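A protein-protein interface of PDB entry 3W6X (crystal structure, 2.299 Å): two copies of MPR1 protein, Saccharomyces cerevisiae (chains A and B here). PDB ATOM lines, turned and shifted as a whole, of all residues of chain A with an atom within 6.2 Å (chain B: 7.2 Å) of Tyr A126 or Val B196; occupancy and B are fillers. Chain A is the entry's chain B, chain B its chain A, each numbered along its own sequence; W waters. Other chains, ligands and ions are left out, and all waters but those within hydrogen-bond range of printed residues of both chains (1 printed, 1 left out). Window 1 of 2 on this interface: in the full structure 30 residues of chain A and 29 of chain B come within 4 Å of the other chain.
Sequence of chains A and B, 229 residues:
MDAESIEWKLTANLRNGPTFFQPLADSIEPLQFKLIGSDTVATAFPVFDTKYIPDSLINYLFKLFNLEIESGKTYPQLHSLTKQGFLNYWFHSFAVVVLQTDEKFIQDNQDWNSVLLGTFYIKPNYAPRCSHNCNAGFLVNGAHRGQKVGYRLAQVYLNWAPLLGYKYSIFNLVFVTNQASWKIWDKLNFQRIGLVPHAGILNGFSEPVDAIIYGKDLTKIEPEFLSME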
ATOM      1  N   LYS A 123     -16.534 -10.900  29.435  1.00  0.00           N
ATOM      2  CA  LYS A 123     -15.213 -10.421  29.848  1.00  0.00           C
ATOM      3  C   LYS A 123     -14.138 -11.220  29.139  1.00  0.00           C
ATOM      4  O   LYS A 123     -14.418 -12.267  28.573  1.00  0.00           O
ATOM      5  CB  LYS A 123     -15.008 -10.568  31.368  1.00  0.00           C
ATOM      6  CG  LYS A 123     -14.870 -12.015  31.807  1.00  0.00           C
ATOM      7  CD  LYS A 123     -14.069 -12.203  33.093  1.00  0.00           C
ATOM      8  CE  LYS A 123     -13.436 -13.607  33.160  1.00  0.00           C
ATOM      9  NZ  LYS A 123     -12.586 -13.833  34.386  1.00  0.00           N
ATOM     10  N   PRO A 124     -12.907 -10.714  29.128  1.00  0.00           N
ATOM     11  CA  PRO A 124     -11.861 -11.546  28.514  1.00  0.00           C
ATOM     12  C   PRO A 124     -11.700 -12.842  29.312  1.00  0.00           C
ATOM     13  O   PRO A 124     -11.734 -12.819  30.537  1.00  0.00           O
ATOM     14  CB  PRO A 124     -10.601 -10.682  28.622  1.00  0.00           C
ATOM     15  CG  PRO A 124     -11.100  -9.252  28.787  1.00  0.00           C
ATOM     16  CD  PRO A 124     -12.443  -9.355  29.482  1.00  0.00           C
ATOM     17  N   ASN A 125     -11.530 -13.962  28.620  1.00  0.00           N
ATOM     18  CA  ASN A 125     -11.272 -15.241  29.264  1.00  0.00           C
ATOM     19  C   ASN A 125      -9.839 -15.428  29.756  1.00  0.00           C
ATOM     20  O   ASN A 125      -9.589 -16.324  30.558  1.00  0.00           O
ATOM     21  CB  ASN A 125     -11.576 -16.382  28.305  1.00  0.00           C
ATOM     22  CG  ASN A 125     -11.804 -17.682  29.027  1.00  0.00           C
ATOM     23  OD1 ASN A 125     -12.499 -17.732  30.048  1.00  0.00           O
ATOM     24  ND2 ASN A 125     -11.188 -18.723  28.543  1.00  0.00           N
ATOM     25  N   TYR A 126      -8.902 -14.623  29.202  1.00  0.00           N
ATOM     26  CA  TYR A 126      -7.483 -14.742  29.454  1.00  0.00           C
ATOM     27  C   TYR A 126      -6.826 -13.371  29.547  1.00  0.00           C
ATOM     28  O   TYR A 126      -7.412 -12.327  29.205  1.00  0.00           O
ATOM     29  CB  TYR A 126      -6.764 -15.453  28.318  1.00  0.00           C
ATOM     30  CG  TYR A 126      -7.289 -16.802  27.900  1.00  0.00           C
ATOM     31  CD1 TYR A 126      -7.061 -17.940  28.675  1.00  0.00           C
ATOM     32  CD2 TYR A 126      -7.961 -16.976  26.678  1.00  0.00           C
ATOM     33  CE1 TYR A 126      -7.505 -19.206  28.265  1.00  0.00           C
ATOM     34  CE2 TYR A 126      -8.421 -18.271  26.263  1.00  0.00           C
ATOM     35  CZ  TYR A 126      -8.186 -19.354  27.072  1.00  0.00           C
ATOM     36  OH  TYR A 126      -8.631 -20.610  26.697  1.00  0.00           O
ATOM     37  N   ALA A 127      -5.576 -13.390  29.972  1.00  0.00           N
ATOM     38  CA  ALA A 127      -4.719 -12.209  29.958  1.00  0.00           C
ATOM     39  C   ALA A 127      -4.499 -11.709  28.486  1.00  0.00           C
ATOM     40  O   ALA A 127      -4.730 -12.460  27.535  1.00  0.00           O
ATOM     41  CB  ALA A 127      -3.387 -12.584  30.651  1.00  0.00           C
ATOM     42  N   PRO A 128      -4.060 -10.438  28.310  1.00  0.00           N
ATOM     43  CA  PRO A 128      -3.994  -9.633  27.059  1.00  0.00           C
ATOM     44  C   PRO A 128      -3.665 -10.309  25.721  1.00  0.00           C
ATOM     45  O   PRO A 128      -4.357  -9.984  24.762  1.00  0.00           O
ATOM     46  CB  PRO A 128      -2.941  -8.574  27.378  1.00  0.00           C
ATOM     47  CG  PRO A 128      -3.191  -8.300  28.842  1.00  0.00           C
ATOM     48  CD  PRO A 128      -3.535  -9.673  29.453  1.00  0.00           C
ATOM     49  N   ARG A 129      -2.682 -11.194  25.621  1.00  0.00           N
ATOM     50  CA  ARG A 129      -2.347 -11.722  24.289  1.00  0.00           C
ATOM     51  C   ARG A 129      -3.426 -12.628  23.744  1.00  0.00           C
ATOM     52  O   ARG A 129      -3.491 -12.894  22.528  1.00  0.00           O
ATOM     53  CB  ARG A 129      -1.046 -12.495  24.307  1.00  0.00           C
ATOM     54  CG  ARG A 129       0.173 -11.601  24.214  1.00  0.00           C
ATOM     55  CD  ARG A 129       1.429 -12.415  24.134  1.00  0.00           C
ATOM     56  NE  ARG A 129       2.559 -11.528  24.283  1.00  0.00           N
ATOM     57  CZ  ARG A 129       3.014 -10.706  23.326  1.00  0.00           C
ATOM     58  NH1 ARG A 129       2.449 -10.674  22.121  1.00  0.00           N
ATOM     59  NH2 ARG A 129       4.048  -9.908  23.590  1.00  0.00           N
ATOM     60  N   CYS A 130      -4.255 -13.130  24.653  1.00  0.00           N
ATOM     61  CA  CYS A 130      -5.338 -14.014  24.273  1.00  0.00           C
ATOM     62  C   CYS A 130      -6.681 -13.402  24.675  1.00  0.00           C
ATOM     63  O   CYS A 130      -7.631 -14.129  24.815  1.00  0.00           O
ATOM     64  CB  CYS A 130      -5.198 -15.385  24.955  1.00  0.00           C
ATOM     65  SG  CYS A 130      -3.627 -16.250  24.660  1.00  0.00           S
ATOM     66  N   SER A 131      -6.745 -12.088  24.885  1.00  0.00           N
ATOM     67  CA  SER A 131      -7.956 -11.471  25.413  1.00  0.00           C
ATOM     68  C   SER A 131      -9.025 -11.219  24.350  1.00  0.00           C
ATOM     69  O   SER A 131     -10.094 -10.694  24.676  1.00  0.00           O
ATOM     70  CB  SER A 131      -7.646 -10.161  26.159  1.00  0.00           C
ATOM     71  OG  SER A 131      -7.105  -9.204  25.278  1.00  0.00           O
ATOM     72  N   ASN A 133     -10.445 -13.682  23.111  1.00  0.00           N
ATOM     73  CA  ASN A 133     -11.409 -14.710  23.528  1.00  0.00           C
ATOM     74  C   ASN A 133     -12.214 -14.224  24.732  1.00  0.00           C
ATOM     75  O   ASN A 133     -11.653 -13.919  25.772  1.00  0.00           O
ATOM     76  CB  ASN A 133     -10.685 -15.997  23.930  1.00  0.00           C
ATOM     77  CG  ASN A 133      -9.757 -16.495  22.852  1.00  0.00           C
ATOM     78  OD1 ASN A 133     -10.183 -17.209  21.932  1.00  0.00           O
ATOM     79  ND2 ASN A 133      -8.466 -16.123  22.950  1.00  0.00           N
ATOM     80  N   TYR A 168     -13.596 -14.669  19.447  1.00  0.00           N
ATOM     81  CA  TYR A 168     -13.870 -16.074  19.746  1.00  0.00           C
ATOM     82  C   TYR A 168     -14.401 -16.168  21.173  1.00  0.00           C
ATOM     83  O   TYR A 168     -13.967 -15.399  22.039  1.00  0.00           O
ATOM     84  CB  TYR A 168     -12.613 -16.933  19.542  1.00  0.00           C
ATOM     85  CG  TYR A 168     -12.868 -18.445  19.410  1.00  0.00           C
ATOM     86  CD1 TYR A 168     -12.904 -19.235  20.529  1.00  0.00           C
ATOM     87  CD2 TYR A 168     -13.034 -19.070  18.167  1.00  0.00           C
ATOM     88  CE1 TYR A 168     -13.123 -20.595  20.439  1.00  0.00           C
ATOM     89  CE2 TYR A 168     -13.235 -20.440  18.051  1.00  0.00           C
ATOM     90  CZ  TYR A 168     -13.279 -21.204  19.209  1.00  0.00           C
ATOM     91  OH  TYR A 168     -13.509 -22.576  19.208  1.00  0.00           O
ATOM     92  N   ILE A 170     -15.359 -18.573  24.638  1.00  0.00           N
ATOM     93  CA  ILE A 170     -14.944 -19.772  25.351  1.00  0.00           C
ATOM     94  C   ILE A 170     -15.754 -19.942  26.623  1.00  0.00           C
ATOM     95  O   ILE A 170     -15.759 -19.036  27.481  1.00  0.00           O
ATOM     96  CB  ILE A 170     -13.500 -19.711  25.832  1.00  0.00           C
ATOM     97  CG1 ILE A 170     -12.551 -19.316  24.725  1.00  0.00           C
ATOM     98  CG2 ILE A 170     -13.073 -21.094  26.381  1.00  0.00           C
ATOM     99  CD1 ILE A 170     -11.917 -20.503  24.092  1.00  0.00           C
ATOM    100  N   ASN A 172     -15.568 -22.282  29.880  1.00  0.00           N
ATOM    101  CA  ASN A 172     -14.573 -23.178  30.416  1.00  0.00           C
ATOM    102  C   ASN A 172     -15.142 -24.455  31.007  1.00  0.00           C
ATOM    103  O   ASN A 172     -14.515 -25.528  30.878  1.00  0.00           O
ATOM    104  CB  ASN A 172     -13.782 -22.448  31.465  1.00  0.00           C
ATOM    105  CG  ASN A 172     -13.165 -21.177  30.921  1.00  0.00           C
ATOM    106  OD1 ASN A 172     -12.237 -21.240  30.090  1.00  0.00           O
ATOM    107  ND2 ASN A 172     -13.648 -20.012  31.402  1.00  0.00           N
ATOM    108  N   ILE A 193     -15.036 -27.994  22.020  1.00  0.00           N
ATOM    109  CA  ILE A 193     -13.621 -28.051  21.702  1.00  0.00           C
ATOM    110  C   ILE A 193     -12.775 -28.749  22.759  1.00  0.00           C
ATOM    111  O   ILE A 193     -11.559 -28.878  22.584  1.00  0.00           O
ATOM    112  CB  ILE A 193     -13.067 -26.662  21.516  1.00  0.00           C
ATOM    113  CG1 ILE A 193     -13.095 -25.923  22.867  1.00  0.00           C
ATOM    114  CG2 ILE A 193     -13.867 -25.926  20.428  1.00  0.00           C
ATOM    115  CD1 ILE A 193     -12.719 -24.472  22.770  1.00  0.00           C
ATOM    116  N   ILE A 213     -15.925 -27.922  27.421  1.00  0.00           N
ATOM    117  CA  ILE A 213     -15.360 -26.659  27.027  1.00  0.00           C
ATOM    118  C   ILE A 213     -15.923 -26.319  25.681  1.00  0.00           C
ATOM    119  O   ILE A 213     -15.673 -27.035  24.712  1.00  0.00           O
ATOM    120  CB  ILE A 213     -13.836 -26.743  26.904  1.00  0.00           C
ATOM    121  CG1 ILE A 213     -13.239 -27.223  28.227  1.00  0.00           C
ATOM    122  CG2 ILE A 213     -13.258 -25.396  26.492  1.00  0.00           C
ATOM    123  CD1 ILE A 213     -11.680 -27.219  28.256  1.00  0.00           C
ATOM    124  N   PRO B  76       0.515 -15.660  28.187  1.00  0.00           N
ATOM    125  CA  PRO B  76      -0.492 -14.774  27.604  1.00  0.00           C
ATOM    126  C   PRO B  76      -0.333 -13.351  28.092  1.00  0.00           C
ATOM    127  O   PRO B  76      -0.950 -12.430  27.551  1.00  0.00           O
ATOM    128  CB  PRO B  76      -1.808 -15.398  28.116  1.00  0.00           C
ATOM    129  CG  PRO B  76      -1.428 -16.019  29.340  1.00  0.00           C
ATOM    130  CD  PRO B  76      -0.081 -16.539  29.211  1.00  0.00           C
ATOM    131  N   ASN B 172      -3.938 -24.696  30.338  1.00  0.00           N
ATOM    132  CA  ASN B 172      -5.011 -24.020  29.594  1.00  0.00           C
ATOM    133  C   ASN B 172      -4.553 -23.577  28.193  1.00  0.00           C
ATOM    134  O   ASN B 172      -5.358 -23.497  27.254  1.00  0.00           O
ATOM    135  CB  ASN B 172      -5.481 -22.806  30.392  1.00  0.00           C
ATOM    136  CG  ASN B 172      -5.960 -23.186  31.793  1.00  0.00           C
ATOM    137  OD1 ASN B 172      -7.007 -23.855  31.936  1.00  0.00           O
ATOM    138  ND2 ASN B 172      -5.180 -22.805  32.844  1.00  0.00           N
ATOM    139  N   LEU B 173      -3.261 -23.324  28.051  1.00  0.00           N
ATOM    140  CA  LEU B 173      -2.788 -22.648  26.890  1.00  0.00           C
ATOM    141  C   LEU B 173      -1.380 -23.097  26.520  1.00  0.00           C
ATOM    142  O   LEU B 173      -0.406 -22.398  26.804  1.00  0.00           O
ATOM    143  CB  LEU B 173      -2.740 -21.145  27.151  1.00  0.00           C
ATOM    144  CG  LEU B 173      -4.015 -20.295  27.147  1.00  0.00           C
ATOM    145  CD1 LEU B 173      -3.677 -18.869  27.642  1.00  0.00           C
ATOM    146  CD2 LEU B 173      -4.632 -20.220  25.781  1.00  0.00           C
ATOM    147  N   PHE B 175       0.751 -23.217  23.496  1.00  0.00           N
ATOM    148  CA  PHE B 175       0.753 -22.799  22.100  1.00  0.00           C
ATOM    149  C   PHE B 175       1.436 -23.843  21.248  1.00  0.00           C
ATOM    150  O   PHE B 175       2.465 -24.383  21.642  1.00  0.00           O
ATOM    151  CB  PHE B 175       1.414 -21.441  21.944  1.00  0.00           C
ATOM    152  CG  PHE B 175       0.709 -20.373  22.705  1.00  0.00           C
ATOM    153  CD1 PHE B 175      -0.528 -19.928  22.297  1.00  0.00           C
ATOM    154  CD2 PHE B 175       1.266 -19.838  23.852  1.00  0.00           C
ATOM    155  CE1 PHE B 175      -1.200 -18.940  23.018  1.00  0.00           C
ATOM    156  CE2 PHE B 175       0.601 -18.852  24.590  1.00  0.00           C
ATOM    157  CZ  PHE B 175      -0.619 -18.401  24.173  1.00  0.00           C
ATOM    158  N   VAL B 176       0.828 -24.152  20.104  1.00  0.00           N
ATOM    159  CA  VAL B 176       1.351 -25.156  19.177  1.00  0.00           C
ATOM    160  C   VAL B 176       2.766 -24.793  18.653  1.00  0.00           C
ATOM    161  O   VAL B 176       3.529 -25.664  18.261  1.00  0.00           O
ATOM    162  CB  VAL B 176       0.403 -25.334  17.977  1.00  0.00           C
ATOM    163  CG1 VAL B 176      -0.950 -25.868  18.432  1.00  0.00           C
ATOM    164  CG2 VAL B 176       0.256 -24.009  17.217  1.00  0.00           C
ATOM    165  N   GLY B 194      -8.237 -30.556  24.554  1.00  0.00           N
ATOM    166  CA  GLY B 194      -8.906 -29.455  23.918  1.00  0.00           C
ATOM    167  C   GLY B 194      -7.999 -28.693  23.007  1.00  0.00           C
ATOM    168  O   GLY B 194      -6.792 -28.808  23.103  1.00  0.00           O
ATOM    169  N   LEU B 195      -8.594 -27.871  22.149  1.00  0.00           N
ATOM    170  CA  LEU B 195      -7.819 -27.083  21.196  1.00  0.00           C
ATOM    171  C   LEU B 195      -8.470 -25.716  21.002  1.00  0.00           C
ATOM    172  O   LEU B 195      -9.594 -25.642  20.531  1.00  0.00           O
ATOM    173  CB  LEU B 195      -7.711 -27.837  19.877  1.00  0.00           C
ATOM    174  CG  LEU B 195      -6.902 -27.074  18.811  1.00  0.00           C
ATOM    175  CD1 LEU B 195      -5.377 -27.034  19.104  1.00  0.00           C
ATOM    176  CD2 LEU B 195      -7.199 -27.680  17.418  1.00  0.00           C
ATOM    177  N   VAL B 196      -7.810 -24.635  21.409  1.00  0.00           N
ATOM    178  CA  VAL B 196      -8.378 -23.304  21.178  1.00  0.00           C
ATOM    179  C   VAL B 196      -7.778 -22.663  19.915  1.00  0.00           C
ATOM    180  O   VAL B 196      -6.559 -22.369  19.861  1.00  0.00           O
ATOM    181  CB  VAL B 196      -8.162 -22.363  22.372  1.00  0.00           C
ATOM    182  CG1 VAL B 196      -8.979 -21.085  22.203  1.00  0.00           C
ATOM    183  CG2 VAL B 196      -8.592 -23.045  23.670  1.00  0.00           C
ATOM    184  N   PRO B 197      -8.620 -22.449  18.882  1.00  0.00           N
ATOM    185  CA  PRO B 197      -8.051 -21.965  17.608  1.00  0.00           C
ATOM    186  C   PRO B 197      -7.755 -20.484  17.701  1.00  0.00           C
ATOM    187  O   PRO B 197      -8.530 -19.746  18.349  1.00  0.00           O
ATOM    188  CB  PRO B 197      -9.141 -22.261  16.578  1.00  0.00           C
ATOM    189  CG  PRO B 197     -10.425 -22.348  17.387  1.00  0.00           C
ATOM    190  CD  PRO B 197     -10.064 -22.696  18.815  1.00  0.00           C
ATOM    191  N   HIS B 198      -6.628 -20.062  17.139  1.00  0.00           N
ATOM    192  CA  HIS B 198      -6.307 -18.629  17.059  1.00  0.00           C
ATOM    193  C   HIS B 198      -6.239 -17.951  18.443  1.00  0.00           C
ATOM    194  O   HIS B 198      -6.435 -16.738  18.566  1.00  0.00           O
ATOM    195  CB  HIS B 198      -7.334 -17.940  16.153  1.00  0.00           C
ATOM    196  CG  HIS B 198      -7.359 -18.487  14.754  1.00  0.00           C
ATOM    197  ND1 HIS B 198      -6.257 -18.452  13.913  1.00  0.00           N
ATOM    198  CD2 HIS B 198      -8.345 -19.091  14.051  1.00  0.00           C
ATOM    199  CE1 HIS B 198      -6.569 -19.002  12.754  1.00  0.00           C
ATOM    200  NE2 HIS B 198      -7.827 -19.397  12.811  1.00  0.00           N
ATOM    201  N   ALA B 199      -5.922 -18.738  19.475  1.00  0.00           N
ATOM    202  CA  ALA B 199      -5.937 -18.282  20.879  1.00  0.00           C
ATOM    203  C   ALA B 199      -5.013 -17.098  21.215  1.00  0.00           C
ATOM    204  O   ALA B 199      -5.438 -16.119  21.818  1.00  0.00           O
ATOM    205  CB  ALA B 199      -5.557 -19.462  21.773  1.00  0.00           C
ATOM    206  N   GLY B 200      -3.742 -17.203  20.833  1.00  0.00           N
ATOM    207  CA  GLY B 200      -2.743 -16.216  21.219  1.00  0.00           C
ATOM    208  C   GLY B 200      -2.189 -15.310  20.106  1.00  0.00           C
ATOM    209  O   GLY B 200      -1.817 -15.757  19.008  1.00  0.00           O
ATOM    210  N   VAL B 209      -2.070 -17.707  17.053  1.00  0.00           N
ATOM    211  CA  VAL B 209      -1.607 -19.088  17.163  1.00  0.00           C
ATOM    212  C   VAL B 209      -2.514 -19.935  18.076  1.00  0.00           C
ATOM    213  O   VAL B 209      -2.943 -19.456  19.153  1.00  0.00           O
ATOM    214  CB  VAL B 209      -0.195 -19.115  17.731  1.00  0.00           C
ATOM    215  CG1 VAL B 209       0.238 -20.539  17.958  1.00  0.00           C
ATOM    216  CG2 VAL B 209       0.774 -18.363  16.780  1.00  0.00           C
ATOM    217  N   ASP B 210      -2.786 -21.172  17.642  1.00  0.00           N
ATOM    218  CA  ASP B 210      -3.639 -22.118  18.363  1.00  0.00           C
ATOM    219  C   ASP B 210      -3.016 -22.524  19.695  1.00  0.00           C
ATOM    220  O   ASP B 210      -1.787 -22.645  19.801  1.00  0.00           O
ATOM    221  CB  ASP B 210      -3.801 -23.424  17.562  1.00  0.00           C
ATOM    222  CG  ASP B 210      -4.682 -23.283  16.321  1.00  0.00           C
ATOM    223  OD1 ASP B 210      -5.406 -22.273  16.172  1.00  0.00           O
ATOM    224  OD2 ASP B 210      -4.661 -24.222  15.496  1.00  0.00           O
ATOM    225  N   ALA B 211      -3.859 -22.806  20.698  1.00  0.00           N
ATOM    226  CA  ALA B 211      -3.368 -23.359  21.960  1.00  0.00           C
ATOM    227  C   ALA B 211      -3.995 -24.702  22.238  1.00  0.00           C
ATOM    228  O   ALA B 211      -5.178 -24.915  22.004  1.00  0.00           O
ATOM    229  CB  ALA B 211      -3.630 -22.407  23.097  1.00  0.00           C
ATOM    230  N   ILE B 212      -3.188 -25.615  22.737  1.00  0.00           N
ATOM    231  CA  ILE B 212      -3.655 -26.937  23.128  1.00  0.00           C
ATOM    232  C   ILE B 212      -3.988 -26.940  24.615  1.00  0.00           C
ATOM    233  O   ILE B 212      -3.263 -26.349  25.418  1.00  0.00           O
ATOM    234  CB  ILE B 212      -2.563 -27.978  22.871  1.00  0.00           C
ATOM    235  CG1 ILE B 212      -2.168 -27.952  21.379  1.00  0.00           C
ATOM    236  CG2 ILE B 212      -2.975 -29.356  23.360  1.00  0.00           C
ATOM    237  CD1 ILE B 212      -0.872 -28.701  21.062  1.00  0.00           C
ATOM    238  N   ILE B 213      -5.084 -27.617  24.964  1.00  0.00           N
ATOM    239  CA  ILE B 213      -5.444 -27.826  26.348  1.00  0.00           C
ATOM    240  C   ILE B 213      -5.025 -29.222  26.782  1.00  0.00           C
ATOM    241  O   ILE B 213      -5.476 -30.214  26.213  1.00  0.00           O
ATOM    242  CB  ILE B 213      -6.953 -27.660  26.582  1.00  0.00           C
ATOM    243  CG1 ILE B 213      -7.422 -26.296  26.062  1.00  0.00           C
ATOM    244  CG2 ILE B 213      -7.250 -27.792  28.044  1.00  0.00           C
ATOM    245  CD1 ILE B 213      -8.930 -26.021  26.268  1.00  0.00           C
HETATM  246  O   HOH W   1      -7.810 -22.754  27.656  1.00  0.00           O
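The backbone NH (N) of Arg A129 lies within hydrogen-bond range of the backbone carbonyl oxygen (O) of Pro B76 (2.9 Å). The backbone NH of Leu B195 sits at hydrogen-bond distance from the backbone carbonyl oxygen of Ile A193 (3.2 Å). O of Ala B199 sits close to SG of Cys A130, 3.4 Å away. O of Ala B199 sits at hydrogen-bond distance from ND2 of Asn A133 (3.2 Å).
Water W1 lies within hydrogen-bond range of the side-chain hydroxyl (OH) of Tyr A126 (2.5 Å) and the backbone carbonyl oxygen (O) of Asn B172 (2.6 Å).
Pro A124 touches none of the printed residues of chain B. Asn A125 touches none of the printed residues of chain B. Of chain B, only Leu B173 and Val B196 come within 4 Å of Tyr A126. Of the printed residues of chain B, Cys A130 touches Pro B76, Leu B173, Phe B175, Ala B199 and Gly B200. Of the printed residues of chain A, Ala B199 touches Arg A129 (3.8 Å), Cys A130 (3.2 Å) and Asn A133 (3.2 Å). The nearest residue of chain B that does not touch Tyr A126 is Asn B172 (4.4 Å). The nearest printed residue of chain B that does not touch Cys A130 is Ala B211 (6.4 Å).
Tyr A126 touches Leu B173 (CD1 to CD1, 3.7 Å). CG2 of Val B196 touches OH of Tyr A126 (3.9 Å). Pro B76 touches Ala A127 (O to C, 3.7 Å). Pro B76 touches Pro A128 (O to N, 3.8 Å). O of Ala B199 touches O of Arg A129, at 3.8 Å. CA of Gly B200 touches O of Arg A129, 3.6 Å away. SG of Cys A130 touches CD1 of Leu B173, at 3.97 Å. Ile A170 touches Val B196 (CD1 to CG1, 3.5 Å). Gly B194 touches Ile A193 (CA to O, 3.0 Å). Ile A213 touches Ile B213 (CD1 to CD1, 3.6 Å).
Ile B213 touches its own counterpart, Ile A213. 2 positions are printed for both chains.
Hydrophobic or aromatic side chains of chain B within 4 Å of the printed part of chain A: Pro B76, Leu B173, Phe B175, Val B196, Pro B197 and Ile B213. Along chain B the printed residues that touch a printed residue of chain A span positions 76 to 213. Printed residues of chain A that touch a printed residue of chain B: Tyr A126, Ala A127, Pro A128, Arg A129, Cys A130, Asn A133, Tyr A168, Ile A170, Ile A193 and Ile A213. Hydrophobic or aromatic side chains of chain A that line the printed part of chain B: Tyr A126, Ala A127, Tyr A168, Ile A170, Ile A193 and Ile A213.
The backbone NH of Val B196 is in hydrogen-bond range of the backbone carbonyl oxygen of Ala B211 (2.7 Å). The backbone NH (N) of Ala B199 sits at hydrogen-bond distance from the backbone carbonyl oxygen (O) of Val B209. N of Val B209 is in hydrogen-bond range of O of Gly B200, 2.8 Å away. N of Asn A125 is in hydrogen-bond range of O of Asn A133 (2.9 Å). O of Pro A128 sits at hydrogen-bond distance from OG of Ser A131 (2.9 Å). The backbone NH (N) of Ile A193 is in hydrogen-bond range of the backbone carbonyl oxygen (O) of Ile A213 (2.9 Å).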
